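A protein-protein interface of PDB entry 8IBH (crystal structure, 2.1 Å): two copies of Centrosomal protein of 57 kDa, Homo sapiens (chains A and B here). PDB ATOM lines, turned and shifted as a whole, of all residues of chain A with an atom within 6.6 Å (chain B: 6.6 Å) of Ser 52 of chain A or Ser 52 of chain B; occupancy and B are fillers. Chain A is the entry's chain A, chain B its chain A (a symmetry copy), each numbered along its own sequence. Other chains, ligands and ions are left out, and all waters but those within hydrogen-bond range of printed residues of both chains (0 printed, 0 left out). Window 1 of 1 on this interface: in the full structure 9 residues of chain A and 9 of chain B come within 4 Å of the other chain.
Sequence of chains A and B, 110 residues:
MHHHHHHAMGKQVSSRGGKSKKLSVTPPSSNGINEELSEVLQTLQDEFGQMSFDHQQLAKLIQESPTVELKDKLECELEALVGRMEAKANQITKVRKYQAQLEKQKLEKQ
Phe 48 of chain A touches Ser 52 of chain B (CE1 to OG, 3.4 Å).
Phe 53 of chain B touches Phe 48 of chain A (N to CE1, 3.5 Å).
Gly 49 of chain A touches Gly 49 of chain B.
Ser 52 of chain A touches Phe 48 of chain B.
Phe 53 of chain A touches Phe 48 of chain B.
Phe 48 of chain A touches Ser 52 of chain B, and with the chains exchanged Ser 52 of chain A touches Phe 48 of chain B.
Phe 48 of chain A touches Phe 53 of chain B, and with the chains exchanged Phe 53 of chain A touches Phe 48 of chain B.
Gly 49 of chain B touches its own counterpart, Gly 49 of chain A.
Ser 52 of chain A touches its own counterpart, Ser 52 of chain B.
Positions printed for both chains: 47, 48, 49, 50, 51, 52, 53, 54, 55, 56, 57, 81 and 85.
Of the 13 printed residues of chain B, 4 touch a printed residue of chain A.
Hydrophobic or aromatic side chains of chain B that line the printed part of chain A: Phe 48.
Of the 13 printed residues of chain A, 4 touch a printed residue of chain B.
Hydrophobic or aromatic side chains of chain A within 4 Å of the printed part of chain B: Phe 48.
Among the printed residues, 6 pairs touch across the chains.
Of chain B, only Phe 48 and Ser 52 come within 4 Å of Ser 52 of chain A.
Printed residues of chain A within 4 Å of Ser 52 of chain B: Phe 48 (3.4 Å) and Ser 52 (3.1 Å).
Printed residues of chain A within 4 Å of Phe 53 of chain B: Phe 48 (3.5 Å).
Printed residues of chain B within 4 Å of Phe 48 of chain A: Ser 52 and Phe 53.
Glu 47 of chain B touches none of the printed residues of chain A.
Glu 47 of chain A touches none of the printed residues of chain B.
The nearest residue of chain B that does not touch Ser 52 of chain A is Gly 49 of chain B (4.5 Å).
The nearest residue of chain A that does not touch Ser 52 of chain B is Gly 49 of chain A (4.5 Å).
The nearest printed residue of chain B that does not touch Gly 49 of chain A is Phe 48 of chain B (4.4 Å).
The side-chain hydroxyl (OG) of Ser 52 of chain A is in hydrogen-bond range of the backbone carbonyl oxygen (O) of Phe 48 of chain A (3.3 Å).
The side-chain hydroxyl (OG) of Ser 52 of chain A lies within hydrogen-bond range of the backbone carbonyl oxygen (O) of Gly 49 of chain A (2.7 Å).
OG of Ser 52 of chain B lies within hydrogen-bond range of O of Phe 48 of chain B (3.3 Å).
OG of Ser 52 of chain B lies within hydrogen-bond range of O of Gly 49 of chain B (2.7 Å).
The side-chain hydroxyl (OG) of Ser 52 of chain A sits at hydrogen-bond distance from the side-chain hydroxyl (OG) of Ser 52 of chain B, 3.1 Å away.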
ATOM      1  N   GLU A  47     -19.035  18.870  -3.523  1.00  0.00           N
ATOM      2  CA  GLU A  47     -19.944  19.396  -4.534  1.00  0.00           C
ATOM      3  C   GLU A  47     -21.148  20.033  -3.849  1.00  0.00           C
ATOM      4  O   GLU A  47     -21.542  21.151  -4.178  1.00  0.00           O
ATOM      5  CB  GLU A  47     -20.387  18.287  -5.490  1.00  0.00           C
ATOM      6  CG  GLU A  47     -19.348  17.946  -6.547  1.00  0.00           C
ATOM      7  CD  GLU A  47     -19.504  16.541  -7.093  1.00  0.00           C
ATOM      8  OE1 GLU A  47     -20.368  15.795  -6.587  1.00  0.00           O
ATOM      9  OE2 GLU A  47     -18.761  16.181  -8.032  1.00  0.00           O
ATOM     10  N   PHE A  48     -21.728  19.313  -2.892  1.00  0.00           N
ATOM     11  CA  PHE A  48     -22.869  19.809  -2.129  1.00  0.00           C
ATOM     12  C   PHE A  48     -22.528  21.170  -1.505  1.00  0.00           C
ATOM     13  O   PHE A  48     -23.372  22.071  -1.473  1.00  0.00           O
ATOM     14  CB  PHE A  48     -23.335  18.794  -1.014  1.00  0.00           C
ATOM     15  CG  PHE A  48     -24.540  19.288  -0.259  1.00  0.00           C
ATOM     16  CD1 PHE A  48     -24.393  20.147   0.789  1.00  0.00           C
ATOM     17  CD2 PHE A  48     -25.832  18.980  -0.667  1.00  0.00           C
ATOM     18  CE1 PHE A  48     -25.519  20.709   1.437  1.00  0.00           C
ATOM     19  CE2 PHE A  48     -26.943  19.562  -0.054  1.00  0.00           C
ATOM     20  CZ  PHE A  48     -26.780  20.383   1.030  1.00  0.00           C
ATOM     21  N   GLY A  49     -21.300  21.321  -0.982  1.00  0.00           N
ATOM     22  CA  GLY A  49     -20.892  22.578  -0.381  1.00  0.00           C
ATOM     23  C   GLY A  49     -20.814  23.721  -1.374  1.00  0.00           C
ATOM     24  O   GLY A  49     -21.277  24.818  -1.088  1.00  0.00           O
ATOM     25  N   GLN A  50     -20.295  23.473  -2.550  1.00  0.00           N
ATOM     26  CA  GLN A  50     -20.227  24.473  -3.589  1.00  0.00           C
ATOM     27  C   GLN A  50     -21.594  24.929  -3.990  1.00  0.00           C
ATOM     28  O   GLN A  50     -21.861  26.067  -4.113  1.00  0.00           O
ATOM     29  CB  GLN A  50     -19.549  23.908  -4.795  1.00  0.00           C
ATOM     30  CG  GLN A  50     -18.296  24.616  -5.064  1.00  0.00           C
ATOM     31  CD  GLN A  50     -17.359  23.815  -5.871  1.00  0.00           C
ATOM     32  OE1 GLN A  50     -16.430  23.229  -5.341  1.00  0.00           O
ATOM     33  NE2 GLN A  50     -17.566  23.809  -7.167  1.00  0.00           N
ATOM     34  N   MET A  51     -22.464  23.982  -4.181  1.00  0.00           N
ATOM     35  CA  MET A  51     -23.828  24.318  -4.551  1.00  0.00           C
ATOM     36  C   MET A  51     -24.545  25.087  -3.449  1.00  0.00           C
ATOM     37  O   MET A  51     -25.318  26.016  -3.724  1.00  0.00           O
ATOM     38  CB  MET A  51     -24.592  23.027  -4.846  1.00  0.00           C
ATOM     39  CG  MET A  51     -24.424  22.363  -6.196  1.00  0.00           C
ATOM     40  SD  MET A  51     -25.422  20.798  -6.158  1.00  0.00           S
ATOM     41  CE  MET A  51     -24.240  19.659  -5.743  1.00  0.00           C
ATOM     42  N   SER A  52     -24.339  24.710  -2.181  1.00  0.00           N
ATOM     43  CA  SER A  52     -25.012  25.453  -1.116  1.00  0.00           C
ATOM     44  C   SER A  52     -24.499  26.889  -1.003  1.00  0.00           C
ATOM     45  O   SER A  52     -25.290  27.828  -0.806  1.00  0.00           O
ATOM     46  CB  SER A  52     -24.850  24.718   0.188  1.00  0.00           C
ATOM     47  OG  SER A  52     -23.449  24.700   0.498  1.00  0.00           O
ATOM     48  N   PHE A  53     -23.202  27.106  -1.183  1.00  0.00           N
ATOM     49  CA  PHE A  53     -22.718  28.481  -1.200  1.00  0.00           C
ATOM     50  C   PHE A  53     -23.321  29.270  -2.361  1.00  0.00           C
ATOM     51  O   PHE A  53     -23.823  30.375  -2.168  1.00  0.00           O
ATOM     52  CB  PHE A  53     -21.218  28.561  -1.311  1.00  0.00           C
ATOM     53  CG  PHE A  53     -20.716  29.960  -1.078  1.00  0.00           C
ATOM     54  CD1 PHE A  53     -20.717  30.488   0.191  1.00  0.00           C
ATOM     55  CD2 PHE A  53     -20.308  30.765  -2.132  1.00  0.00           C
ATOM     56  CE1 PHE A  53     -20.283  31.767   0.409  1.00  0.00           C
ATOM     57  CE2 PHE A  53     -19.842  32.053  -1.882  1.00  0.00           C
ATOM     58  CZ  PHE A  53     -19.857  32.541  -0.627  1.00  0.00           C
ATOM     59  N   ASP A  54     -23.297  28.681  -3.578  1.00  0.00           N
ATOM     60  CA  ASP A  54     -23.984  29.273  -4.724  1.00  0.00           C
ATOM     61  C   ASP A  54     -25.443  29.581  -4.393  1.00  0.00           C
ATOM     62  O   ASP A  54     -25.939  30.658  -4.719  1.00  0.00           O
ATOM     63  CB  ASP A  54     -23.882  28.336  -5.942  1.00  0.00           C
ATOM     64  CG  ASP A  54     -22.455  28.259  -6.513  1.00  0.00           C
ATOM     65  OD1 ASP A  54     -21.518  28.945  -5.993  1.00  0.00           O
ATOM     66  OD2 ASP A  54     -22.244  27.507  -7.510  1.00  0.00           O
ATOM     67  N   HIS A  55     -26.120  28.678  -3.690  1.00  0.00           N
ATOM     68  CA  HIS A  55     -27.528  28.897  -3.362  1.00  0.00           C
ATOM     69  C   HIS A  55     -27.689  30.096  -2.434  1.00  0.00           C
ATOM     70  O   HIS A  55     -28.563  30.954  -2.648  1.00  0.00           O
ATOM     71  CB  HIS A  55     -28.108  27.607  -2.749  1.00  0.00           C
ATOM     72  CG  HIS A  55     -29.487  27.764  -2.220  1.00  0.00           C
ATOM     73  ND1 HIS A  55     -30.611  27.389  -2.938  1.00  0.00           N
ATOM     74  CD2 HIS A  55     -29.945  28.306  -1.068  1.00  0.00           C
ATOM     75  CE1 HIS A  55     -31.693  27.661  -2.232  1.00  0.00           C
ATOM     76  NE2 HIS A  55     -31.318  28.259  -1.114  1.00  0.00           N
ATOM     77  N   GLN A  56     -26.800  30.228  -1.442  1.00  0.00           N
ATOM     78  CA  GLN A  56     -26.881  31.365  -0.525  1.00  0.00           C
ATOM     79  C   GLN A  56     -26.588  32.677  -1.247  1.00  0.00           C
ATOM     80  O   GLN A  56     -27.222  33.701  -0.982  1.00  0.00           O
ATOM     81  CB  GLN A  56     -25.911  31.139   0.651  1.00  0.00           C
ATOM     82  CG  GLN A  56     -26.079  32.085   1.758  1.00  0.00           C
ATOM     83  CD  GLN A  56     -25.128  33.281   1.607  1.00  0.00           C
ATOM     84  OE1 GLN A  56     -24.155  33.201   0.877  1.00  0.00           O
ATOM     85  NE2 GLN A  56     -25.423  34.386   2.290  1.00  0.00           N
ATOM     86  N   GLN A  57     -25.631  32.675  -2.167  1.00  0.00           N
ATOM     87  CA  GLN A  57     -25.345  33.894  -2.919  1.00  0.00           C
ATOM     88  C   GLN A  57     -26.529  34.299  -3.807  1.00  0.00           C
ATOM     89  O   GLN A  57     -26.907  35.462  -3.852  1.00  0.00           O
ATOM     90  CB  GLN A  57     -24.106  33.621  -3.754  1.00  0.00           C
ATOM     91  CG  GLN A  57     -22.796  34.112  -3.201  1.00  0.00           C
ATOM     92  CD  GLN A  57     -21.645  33.761  -4.166  1.00  0.00           C
ATOM     93  OE1 GLN A  57     -21.318  32.591  -4.430  1.00  0.00           O
ATOM     94  NE2 GLN A  57     -21.065  34.795  -4.731  1.00  0.00           N
ATOM     95  N   LEU A  81     -31.012  24.669  -8.586  1.00  0.00           N
ATOM     96  CA  LEU A  81     -29.988  24.336  -7.608  1.00  0.00           C
ATOM     97  C   LEU A  81     -30.576  23.559  -6.436  1.00  0.00           C
ATOM     98  O   LEU A  81     -29.915  22.653  -5.876  1.00  0.00           O
ATOM     99  CB  LEU A  81     -29.330  25.606  -7.098  1.00  0.00           C
ATOM    100  CG  LEU A  81     -27.830  25.612  -6.859  1.00  0.00           C
ATOM    101  CD1 LEU A  81     -26.985  24.921  -7.930  1.00  0.00           C
ATOM    102  CD2 LEU A  81     -27.416  27.133  -6.749  1.00  0.00           C
ATOM    103  N   MET A  85     -29.336  19.940  -5.191  1.00  0.00           N
ATOM    104  CA  MET A  85     -28.817  19.784  -3.834  1.00  0.00           C
ATOM    105  C   MET A  85     -29.530  18.644  -3.113  1.00  0.00           C
ATOM    106  O   MET A  85     -28.929  17.915  -2.315  1.00  0.00           O
ATOM    107  CB  MET A  85     -29.004  21.065  -3.015  1.00  0.00           C
ATOM    108  CG  MET A  85     -27.925  22.155  -3.284  1.00  0.00           C
ATOM    109  SD  MET A  85     -28.175  23.717  -2.423  1.00  0.00           S
ATOM    110  CE  MET A  85     -28.156  23.317  -0.768  1.00  0.00           C
ATOM    111  N   GLU B  47     -15.888  24.355   5.590  1.00  0.00           N
ATOM    112  CA  GLU B  47     -16.676  24.451   6.812  1.00  0.00           C
ATOM    113  C   GLU B  47     -18.120  24.786   6.458  1.00  0.00           C
ATOM    114  O   GLU B  47     -19.053  24.153   6.952  1.00  0.00           O
ATOM    115  CB  GLU B  47     -16.088  25.507   7.750  1.00  0.00           C
ATOM    116  CG  GLU B  47     -14.874  25.022   8.526  1.00  0.00           C
ATOM    117  CD  GLU B  47     -13.975  26.154   8.980  1.00  0.00           C
ATOM    118  OE1 GLU B  47     -14.248  27.317   8.615  1.00  0.00           O
ATOM    119  OE2 GLU B  47     -12.993  25.882   9.704  1.00  0.00           O
ATOM    120  N   PHE B  48     -18.297  25.783   5.595  1.00  0.00           N
ATOM    121  CA  PHE B  48     -19.622  26.191   5.139  1.00  0.00           C
ATOM    122  C   PHE B  48     -20.374  24.981   4.566  1.00  0.00           C
ATOM    123  O   PHE B  48     -21.579  24.832   4.791  1.00  0.00           O
ATOM    124  CB  PHE B  48     -19.561  27.354   4.075  1.00  0.00           C
ATOM    125  CG  PHE B  48     -20.930  27.805   3.641  1.00  0.00           C
ATOM    126  CD1 PHE B  48     -21.597  27.136   2.658  1.00  0.00           C
ATOM    127  CD2 PHE B  48     -21.600  28.832   4.294  1.00  0.00           C
ATOM    128  CE1 PHE B  48     -22.929  27.475   2.316  1.00  0.00           C
ATOM    129  CE2 PHE B  48     -22.926  29.144   3.984  1.00  0.00           C
ATOM    130  CZ  PHE B  48     -23.564  28.497   2.959  1.00  0.00           C
ATOM    131  N   GLY B  49     -19.676  24.123   3.803  1.00  0.00           N
ATOM    132  CA  GLY B  49     -20.307  22.948   3.230  1.00  0.00           C
ATOM    133  C   GLY B  49     -20.762  21.944   4.270  1.00  0.00           C
ATOM    134  O   GLY B  49     -21.866  21.421   4.179  1.00  0.00           O
ATOM    135  N   GLN B  50     -19.965  21.709   5.283  1.00  0.00           N
ATOM    136  CA  GLN B  50     -20.327  20.817   6.357  1.00  0.00           C
ATOM    137  C   GLN B  50     -21.541  21.307   7.081  1.00  0.00           C
ATOM    138  O   GLN B  50     -22.438  20.596   7.349  1.00  0.00           O
ATOM    139  CB  GLN B  50     -19.205  20.721   7.339  1.00  0.00           C
ATOM    140  CG  GLN B  50     -18.672  19.358   7.386  1.00  0.00           C
ATOM    141  CD  GLN B  50     -17.294  19.310   7.904  1.00  0.00           C
ATOM    142  OE1 GLN B  50     -16.348  19.210   7.140  1.00  0.00           O
ATOM    143  NE2 GLN B  50     -17.161  19.345   9.210  1.00  0.00           N
ATOM    144  N   MET B  51     -21.540  22.573   7.380  1.00  0.00           N
ATOM    145  CA  MET B  51     -22.682  23.156   8.063  1.00  0.00           C
ATOM    146  C   MET B  51     -23.941  23.111   7.206  1.00  0.00           C
ATOM    147  O   MET B  51     -25.045  22.871   7.716  1.00  0.00           O
ATOM    148  CB  MET B  51     -22.359  24.608   8.412  1.00  0.00           C
ATOM    149  CG  MET B  51     -21.518  24.903   9.637  1.00  0.00           C
ATOM    150  SD  MET B  51     -21.267  26.741   9.692  1.00  0.00           S
ATOM    151  CE  MET B  51     -19.756  26.893   8.941  1.00  0.00           C
ATOM    152  N   SER B  52     -23.823  23.370   5.898  1.00  0.00           N
ATOM    153  CA  SER B  52     -25.025  23.315   5.067  1.00  0.00           C
ATOM    154  C   SER B  52     -25.586  21.897   4.960  1.00  0.00           C
ATOM    155  O   SER B  52     -26.813  21.697   5.015  1.00  0.00           O
ATOM    156  CB  SER B  52     -24.719  23.878   3.705  1.00  0.00           C
ATOM    157  OG  SER B  52     -23.740  23.023   3.098  1.00  0.00           O
ATOM    158  N   PHE B  53     -24.727  20.888   4.871  1.00  0.00           N
ATOM    159  CA  PHE B  53     -25.243  19.525   4.892  1.00  0.00           C
ATOM    160  C   PHE B  53     -25.940  19.212   6.215  1.00  0.00           C
ATOM    161  O   PHE B  53     -27.057  18.702   6.224  1.00  0.00           O
ATOM    162  CB  PHE B  53     -24.161  18.498   4.681  1.00  0.00           C
ATOM    163  CG  PHE B  53     -24.733  17.125   4.457  1.00  0.00           C
ATOM    164  CD1 PHE B  53     -25.346  16.821   3.265  1.00  0.00           C
ATOM    165  CD2 PHE B  53     -24.716  16.164   5.458  1.00  0.00           C
ATOM    166  CE1 PHE B  53     -25.888  15.582   3.060  1.00  0.00           C
ATOM    167  CE2 PHE B  53     -25.247  14.900   5.216  1.00  0.00           C
ATOM    168  CZ  PHE B  53     -25.842  14.636   4.038  1.00  0.00           C
ATOM    169  N   ASP B  54     -25.283  19.552   7.347  1.00  0.00           N
ATOM    170  CA  ASP B  54     -25.919  19.445   8.659  1.00  0.00           C
ATOM    171  C   ASP B  54     -27.265  20.166   8.677  1.00  0.00           C
ATOM    172  O   ASP B  54     -28.248  19.631   9.187  1.00  0.00           O
ATOM    173  CB  ASP B  54     -24.982  20.001   9.747  1.00  0.00           C
ATOM    174  CG  ASP B  54     -23.755  19.105   9.987  1.00  0.00           C
ATOM    175  OD1 ASP B  54     -23.612  18.023   9.332  1.00  0.00           O
ATOM    176  OD2 ASP B  54     -22.903  19.467  10.851  1.00  0.00           O
ATOM    177  N   HIS B  55     -27.343  21.345   8.069  1.00  0.00           N
ATOM    178  CA  HIS B  55     -28.594  22.102   8.072  1.00  0.00           C
ATOM    179  C   HIS B  55     -29.679  21.359   7.300  1.00  0.00           C
ATOM    180  O   HIS B  55     -30.825  21.242   7.765  1.00  0.00           O
ATOM    181  CB  HIS B  55     -28.333  23.508   7.499  1.00  0.00           C
ATOM    182  CG  HIS B  55     -29.567  24.310   7.296  1.00  0.00           C
ATOM    183  ND1 HIS B  55     -30.003  25.257   8.208  1.00  0.00           N
ATOM    184  CD2 HIS B  55     -30.501  24.278   6.317  1.00  0.00           C
ATOM    185  CE1 HIS B  55     -31.130  25.795   7.777  1.00  0.00           C
ATOM    186  NE2 HIS B  55     -31.476  25.186   6.655  1.00  0.00           N
ATOM    187  N   GLN B  56     -29.321  20.770   6.152  1.00  0.00           N
ATOM    188  CA  GLN B  56     -30.305  20.024   5.367  1.00  0.00           C
ATOM    189  C   GLN B  56     -30.769  18.775   6.111  1.00  0.00           C
ATOM    190  O   GLN B  56     -31.948  18.415   6.072  1.00  0.00           O
ATOM    191  CB  GLN B  56     -29.699  19.672   3.995  1.00  0.00           C
ATOM    192  CG  GLN B  56     -30.666  19.142   3.030  1.00  0.00           C
ATOM    193  CD  GLN B  56     -30.694  17.607   3.065  1.00  0.00           C
ATOM    194  OE1 GLN B  56     -29.765  16.990   3.558  1.00  0.00           O
ATOM    195  NE2 GLN B  56     -31.765  17.003   2.553  1.00  0.00           N
ATOM    196  N   GLN B  57     -29.861  18.093   6.798  1.00  0.00           N
ATOM    197  CA  GLN B  57     -30.263  16.916   7.565  1.00  0.00           C
ATOM    198  C   GLN B  57     -31.205  17.291   8.718  1.00  0.00           C
ATOM    199  O   GLN B  57     -32.216  16.637   8.936  1.00  0.00           O
ATOM    200  CB  GLN B  57     -28.993  16.269   8.087  1.00  0.00           C
ATOM    201  CG  GLN B  57     -28.457  15.101   7.304  1.00  0.00           C
ATOM    202  CD  GLN B  57     -27.174  14.560   7.966  1.00  0.00           C
ATOM    203  OE1 GLN B  57     -26.129  15.227   8.058  1.00  0.00           O
ATOM    204  NE2 GLN B  57     -27.282  13.353   8.471  1.00  0.00           N
ATOM    205  N   LEU B  81     -27.340  27.147  13.573  1.00  0.00           N
ATOM    206  CA  LEU B  81     -26.584  26.827  12.374  1.00  0.00           C
ATOM    207  C   LEU B  81     -26.776  27.890  11.300  1.00  0.00           C
ATOM    208  O   LEU B  81     -25.831  28.208  10.539  1.00  0.00           O
ATOM    209  CB  LEU B  81     -27.017  25.475  11.836  1.00  0.00           C
ATOM    210  CG  LEU B  81     -25.965  24.533  11.278  1.00  0.00           C
ATOM    211  CD1 LEU B  81     -24.667  24.438  12.082  1.00  0.00           C
ATOM    212  CD2 LEU B  81     -26.652  23.112  11.203  1.00  0.00           C
ATOM    213  N   MET B  85     -23.822  29.972   9.531  1.00  0.00           N
ATOM    214  CA  MET B  85     -23.633  29.869   8.087  1.00  0.00           C
ATOM    215  C   MET B  85     -23.590  31.253   7.448  1.00  0.00           C
ATOM    216  O   MET B  85     -22.853  31.492   6.484  1.00  0.00           O
ATOM    217  CB  MET B  85     -24.765  29.071   7.432  1.00  0.00           C
ATOM    218  CG  MET B  85     -24.605  27.526   7.546  1.00  0.00           C
ATOM    219  SD  MET B  85     -25.973  26.557   6.887  1.00  0.00           S
ATOM    220  CE  MET B  85     -26.062  26.984   5.241  1.00  0.00           C
